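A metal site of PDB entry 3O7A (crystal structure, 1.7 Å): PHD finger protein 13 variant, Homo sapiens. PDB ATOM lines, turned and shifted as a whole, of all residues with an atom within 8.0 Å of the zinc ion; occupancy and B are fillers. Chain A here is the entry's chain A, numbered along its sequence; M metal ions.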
ATOM      1  N   VAL A   5     -20.851 -21.675 -19.674  1.00  0.00           N
ATOM      2  CA  VAL A   5     -19.913 -20.591 -19.255  1.00  0.00           C
ATOM      3  C   VAL A   5     -18.526 -20.864 -19.810  1.00  0.00           C
ATOM      4  O   VAL A   5     -17.932 -21.939 -19.557  1.00  0.00           O
ATOM      5  CB  VAL A   5     -19.833 -20.461 -17.720  1.00  0.00           C
ATOM      6  CG1 VAL A   5     -18.859 -19.383 -17.347  1.00  0.00           C
ATOM      7  CG2 VAL A   5     -21.247 -20.063 -17.160  1.00  0.00           C
ATOM      8  N   THR A   6     -17.984 -19.859 -20.531  1.00  0.00           N
ATOM      9  CA  THR A   6     -16.623 -19.949 -21.090  1.00  0.00           C
ATOM     10  C   THR A   6     -15.838 -18.700 -20.859  1.00  0.00           C
ATOM     11  O   THR A   6     -14.604 -18.757 -20.738  1.00  0.00           O
ATOM     12  CB  THR A   6     -16.633 -20.266 -22.574  1.00  0.00           C
ATOM     13  OG1 THR A   6     -17.338 -19.248 -23.341  1.00  0.00           O
ATOM     14  CG2 THR A   6     -17.345 -21.605 -22.796  1.00  0.00           C
ATOM     15  N   CYS A   7     -16.501 -17.559 -20.873  1.00  0.00           N
ATOM     16  CA  CYS A   7     -15.792 -16.275 -20.783  1.00  0.00           C
ATOM     17  C   CYS A   7     -15.190 -16.056 -19.399  1.00  0.00           C
ATOM     18  O   CYS A   7     -15.709 -16.628 -18.401  1.00  0.00           O
ATOM     19  CB  CYS A   7     -16.803 -15.162 -21.053  1.00  0.00           C
ATOM     20  SG  CYS A   7     -16.062 -13.496 -21.231  1.00  0.00           S
ATOM     21  N   PHE A   8     -14.155 -15.208 -19.302  1.00  0.00           N
ATOM     22  CA  PHE A   8     -13.550 -14.955 -17.992  1.00  0.00           C
ATOM     23  C   PHE A   8     -14.453 -14.203 -17.026  1.00  0.00           C
ATOM     24  O   PHE A   8     -14.179 -14.150 -15.851  1.00  0.00           O
ATOM     25  CB  PHE A   8     -12.195 -14.217 -18.144  1.00  0.00           C
ATOM     26  CG  PHE A   8     -12.260 -13.053 -19.039  1.00  0.00           C
ATOM     27  CD1 PHE A   8     -12.837 -11.826 -18.580  1.00  0.00           C
ATOM     28  CD2 PHE A   8     -11.755 -13.126 -20.356  1.00  0.00           C
ATOM     29  CE1 PHE A   8     -12.988 -10.742 -19.428  1.00  0.00           C
ATOM     30  CE2 PHE A   8     -11.835 -11.982 -21.197  1.00  0.00           C
ATOM     31  CZ  PHE A   8     -12.481 -10.829 -20.746  1.00  0.00           C
ATOM     32  N   CYS A   9     -15.568 -13.668 -17.508  1.00  0.00           N
ATOM     33  CA  CYS A   9     -16.516 -13.060 -16.603  1.00  0.00           C
ATOM     34  C   CYS A   9     -17.347 -14.081 -15.814  1.00  0.00           C
ATOM     35  O   CYS A   9     -17.986 -13.709 -14.825  1.00  0.00           O
ATOM     36  CB  CYS A   9     -17.483 -12.121 -17.360  1.00  0.00           C
ATOM     37  SG  CYS A   9     -18.640 -13.002 -18.434  1.00  0.00           S
ATOM     38  N   MET A  10     -17.195 -15.352 -16.159  1.00  0.00           N
ATOM     39  CA  MET A  10     -17.838 -16.448 -15.449  1.00  0.00           C
ATOM     40  C   MET A  10     -19.364 -16.427 -15.636  1.00  0.00           C
ATOM     41  O   MET A  10     -20.098 -17.090 -14.856  1.00  0.00           O
ATOM     42  CB  MET A  10     -17.534 -16.388 -13.933  1.00  0.00           C
ATOM     43  CG  MET A  10     -16.071 -16.270 -13.614  1.00  0.00           C
ATOM     44  SD  MET A  10     -15.262 -17.797 -14.128  1.00  0.00           S
ATOM     45  CE  MET A  10     -15.578 -18.749 -12.623  1.00  0.00           C
ATOM     46  N   LYS A  11     -19.860 -15.677 -16.653  1.00  0.00           N
ATOM     47  CA  LYS A  11     -21.311 -15.637 -16.959  1.00  0.00           C
ATOM     48  C   LYS A  11     -21.552 -16.381 -18.305  1.00  0.00           C
ATOM     49  O   LYS A  11     -20.642 -16.498 -19.144  1.00  0.00           O
ATOM     50  CB  LYS A  11     -21.832 -14.178 -17.036  1.00  0.00           C
ATOM     51  CG  LYS A  11     -21.557 -13.404 -15.740  1.00  0.00           C
ATOM     52  CD  LYS A  11     -22.227 -12.084 -15.772  1.00  0.00           C
ATOM     53  CE  LYS A  11     -22.022 -11.347 -14.486  1.00  0.00           C
ATOM     54  NZ  LYS A  11     -22.802 -10.078 -14.496  1.00  0.00           N
ATOM     55  N   PRO A  12     -22.741 -16.937 -18.483  1.00  0.00           N
ATOM     56  CA  PRO A  12     -22.987 -17.826 -19.627  1.00  0.00           C
ATOM     57  C   PRO A  12     -23.069 -17.087 -20.997  1.00  0.00           C
ATOM     58  O   PRO A  12     -23.249 -15.877 -21.048  1.00  0.00           O
ATOM     59  CB  PRO A  12     -24.368 -18.431 -19.284  1.00  0.00           C
ATOM     60  CG  PRO A  12     -24.966 -17.573 -18.308  1.00  0.00           C
ATOM     61  CD  PRO A  12     -23.847 -16.980 -17.490  1.00  0.00           C
ATOM     62  N   PHE A  13     -23.057 -17.887 -22.086  1.00  0.00           N
ATOM     63  CA  PHE A  13     -23.356 -17.396 -23.414  1.00  0.00           C
ATOM     64  C   PHE A  13     -24.650 -16.558 -23.480  1.00  0.00           C
ATOM     65  O   PHE A  13     -24.595 -15.401 -23.841  1.00  0.00           O
ATOM     66  CB  PHE A  13     -23.440 -18.629 -24.335  1.00  0.00           C
ATOM     67  CG  PHE A  13     -24.050 -18.373 -25.662  1.00  0.00           C
ATOM     68  CD1 PHE A  13     -23.696 -17.269 -26.412  1.00  0.00           C
ATOM     69  CD2 PHE A  13     -24.899 -19.320 -26.224  1.00  0.00           C
ATOM     70  CE1 PHE A  13     -24.232 -17.056 -27.699  1.00  0.00           C
ATOM     71  CE2 PHE A  13     -25.425 -19.120 -27.506  1.00  0.00           C
ATOM     72  CZ  PHE A  13     -25.081 -18.013 -28.237  1.00  0.00           C
ATOM     73  N   ARG A  16     -25.562 -14.019 -26.275  1.00  0.00           N
ATOM     74  CA  ARG A  16     -24.844 -12.759 -26.443  1.00  0.00           C
ATOM     75  C   ARG A  16     -23.803 -12.918 -27.532  1.00  0.00           C
ATOM     76  O   ARG A  16     -23.302 -14.024 -27.730  1.00  0.00           O
ATOM     77  CB  ARG A  16     -24.183 -12.414 -25.106  1.00  0.00           C
ATOM     78  CG  ARG A  16     -25.168 -12.075 -24.024  1.00  0.00           C
ATOM     79  CD  ARG A  16     -24.516 -12.071 -22.653  1.00  0.00           C
ATOM     80  NE  ARG A  16     -23.475 -11.035 -22.558  1.00  0.00           N
ATOM     81  CZ  ARG A  16     -22.607 -10.940 -21.551  1.00  0.00           C
ATOM     82  NH1 ARG A  16     -22.731 -11.698 -20.489  1.00  0.00           N
ATOM     83  NH2 ARG A  16     -21.677  -9.982 -21.575  1.00  0.00           N
ATOM     84  N   PRO A  17     -23.467 -11.856 -28.242  1.00  0.00           N
ATOM     85  CA  PRO A  17     -22.318 -11.959 -29.225  1.00  0.00           C
ATOM     86  C   PRO A  17     -21.004 -12.382 -28.522  1.00  0.00           C
ATOM     87  O   PRO A  17     -20.648 -11.828 -27.498  1.00  0.00           O
ATOM     88  CB  PRO A  17     -22.163 -10.538 -29.794  1.00  0.00           C
ATOM     89  CG  PRO A  17     -23.365  -9.758 -29.268  1.00  0.00           C
ATOM     90  CD  PRO A  17     -24.028 -10.488 -28.128  1.00  0.00           C
ATOM     91  N   MET A  18     -20.294 -13.323 -29.126  1.00  0.00           N
ATOM     92  CA  MET A  18     -19.046 -13.837 -28.577  1.00  0.00           C
ATOM     93  C   MET A  18     -18.042 -14.030 -29.676  1.00  0.00           C
ATOM     94  O   MET A  18     -18.401 -14.045 -30.851  1.00  0.00           O
ATOM     95  CB  MET A  18     -19.293 -15.164 -27.899  1.00  0.00           C
ATOM     96  CG  MET A  18     -20.295 -15.057 -26.706  1.00  0.00           C
ATOM     97  SD  MET A  18     -20.309 -16.529 -25.656  1.00  0.00           S
ATOM     98  CE  MET A  18     -18.898 -16.205 -24.615  1.00  0.00           C
ATOM     99  N   TRP A  27     -14.167 -18.953 -25.938  1.00  0.00           N
ATOM    100  CA  TRP A  27     -15.214 -18.006 -26.365  1.00  0.00           C
ATOM    101  C   TRP A  27     -15.382 -16.896 -25.299  1.00  0.00           C
ATOM    102  O   TRP A  27     -15.610 -17.190 -24.129  1.00  0.00           O
ATOM    103  CB  TRP A  27     -16.563 -18.748 -26.535  1.00  0.00           C
ATOM    104  CG  TRP A  27     -16.654 -19.536 -27.791  1.00  0.00           C
ATOM    105  CD1 TRP A  27     -16.518 -20.916 -27.942  1.00  0.00           C
ATOM    106  CD2 TRP A  27     -16.882 -19.016 -29.085  1.00  0.00           C
ATOM    107  NE1 TRP A  27     -16.673 -21.250 -29.264  1.00  0.00           N
ATOM    108  CE2 TRP A  27     -16.899 -20.105 -29.988  1.00  0.00           C
ATOM    109  CE3 TRP A  27     -17.095 -17.737 -29.565  1.00  0.00           C
ATOM    110  CZ2 TRP A  27     -17.163 -19.936 -31.345  1.00  0.00           C
ATOM    111  CZ3 TRP A  27     -17.347 -17.574 -30.924  1.00  0.00           C
ATOM    112  CH2 TRP A  27     -17.339 -18.668 -31.806  1.00  0.00           C
ATOM    113  N   ILE A  28     -15.270 -15.648 -25.738  1.00  0.00           N
ATOM    114  CA  ILE A  28     -15.342 -14.474 -24.878  1.00  0.00           C
ATOM    115  C   ILE A  28     -16.459 -13.568 -25.357  1.00  0.00           C
ATOM    116  O   ILE A  28     -16.683 -13.412 -26.556  1.00  0.00           O
ATOM    117  CB  ILE A  28     -13.977 -13.657 -25.021  1.00  0.00           C
ATOM    118  CG1 ILE A  28     -12.758 -14.563 -24.747  1.00  0.00           C
ATOM    119  CG2 ILE A  28     -13.991 -12.366 -24.202  1.00  0.00           C
ATOM    120  CD1 ILE A  28     -12.753 -15.125 -23.392  1.00  0.00           C
ATOM    121  N   HIS A  29     -17.216 -12.972 -24.423  1.00  0.00           N
ATOM    122  CA  HIS A  29     -18.269 -12.031 -24.878  1.00  0.00           C
ATOM    123  C   HIS A  29     -17.614 -10.795 -25.512  1.00  0.00           C
ATOM    124  O   HIS A  29     -16.574 -10.317 -25.029  1.00  0.00           O
ATOM    125  CB  HIS A  29     -19.092 -11.529 -23.662  1.00  0.00           C
ATOM    126  CG  HIS A  29     -19.839 -12.596 -22.955  1.00  0.00           C
ATOM    127  ND1 HIS A  29     -19.460 -13.058 -21.693  1.00  0.00           N
ATOM    128  CD2 HIS A  29     -20.920 -13.344 -23.338  1.00  0.00           C
ATOM    129  CE1 HIS A  29     -20.316 -13.995 -21.310  1.00  0.00           C
ATOM    130  NE2 HIS A  29     -21.167 -14.225 -22.303  1.00  0.00           N
ATOM    131  N   LEU A  30     -18.198 -10.317 -26.591  1.00  0.00           N
ATOM    132  CA  LEU A  30     -17.736  -9.051 -27.212  1.00  0.00           C
ATOM    133  C   LEU A  30     -17.646  -7.940 -26.177  1.00  0.00           C
ATOM    134  O   LEU A  30     -16.657  -7.196 -26.103  1.00  0.00           O
ATOM    135  CB  LEU A  30     -18.699  -8.644 -28.319  1.00  0.00           C
ATOM    136  CG  LEU A  30     -18.169  -8.996 -29.696  1.00  0.00           C
ATOM    137  CD1 LEU A  30     -17.935 -10.442 -29.933  1.00  0.00           C
ATOM    138  CD2 LEU A  30     -19.029  -8.296 -30.794  1.00  0.00           C
ATOM    139  N   SER A  31     -18.667  -7.818 -25.324  1.00  0.00           N
ATOM    140  CA  SER A  31     -18.653  -6.706 -24.338  1.00  0.00           C
ATOM    141  C   SER A  31     -17.475  -6.807 -23.403  1.00  0.00           C
ATOM    142  O   SER A  31     -16.759  -5.822 -23.126  1.00  0.00           O
ATOM    143  CB  SER A  31     -19.978  -6.619 -23.574  1.00  0.00           C
ATOM    144  OG  SER A  31     -20.079  -7.786 -22.753  1.00  0.00           O
ATOM    145  N   CYS A  32     -17.206  -8.021 -22.932  1.00  0.00           N
ATOM    146  CA  CYS A  32     -16.100  -8.237 -22.012  1.00  0.00           C
ATOM    147  C   CYS A  32     -14.758  -7.910 -22.651  1.00  0.00           C
ATOM    148  O   CYS A  32     -13.818  -7.467 -21.959  1.00  0.00           O
ATOM    149  CB  CYS A  32     -16.148  -9.688 -21.527  1.00  0.00           C
ATOM    150  SG  CYS A  32     -17.647 -10.038 -20.579  1.00  0.00           S
ATOM    151  N   ALA A  33     -14.656  -8.212 -23.926  1.00  0.00           N
ATOM    152  CA  ALA A  33     -13.436  -8.006 -24.697  1.00  0.00           C
ATOM    153  C   ALA A  33     -13.283  -6.558 -25.142  1.00  0.00           C
ATOM    154  O   ALA A  33     -12.266  -6.222 -25.817  1.00  0.00           O
ATOM    155  CB  ALA A  33     -13.448  -8.900 -25.910  1.00  0.00           C
HETATM  156 ZN    ZN M   1     -17.894 -12.308 -20.507  1.00  0.00          ZN
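A ring nitrogen (NE2) of His 29 sits close to the guanidinium group of Arg 16, at 3.5 Å.
The backbone carbonyl oxygen (O) of Pro 12 lies within hydrogen-bond range of a ring nitrogen (NE2) of His 29 (2.9 Å).
The backbone carbonyl oxygen of Trp 27 sits at hydrogen-bond distance from the backbone NH of Cys 7 (3.4 Å).
SG of Cys 9 lies close to N of Lys 11, 3.4 Å away.
Within 4 Å of the zinc ion: Cys 7, Cys 9, His 29 and Cys 32.
Along chain A the residues within 4 Å of the zinc ion span positions 7 to 32.
The nearest printed residue that does not touch the zinc ion is Arg 16 (4.6 Å).
The zinc ion is bound by a ring nitrogen (ND1) of His 29 (2.1 Å), the side-chain sulfur (SG) of Cys 32 (2.3 Å), the side-chain sulfur (SG) of Cys 7 (2.3 Å) and the side-chain sulfur (SG) of Cys 9 (2.3 Å).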
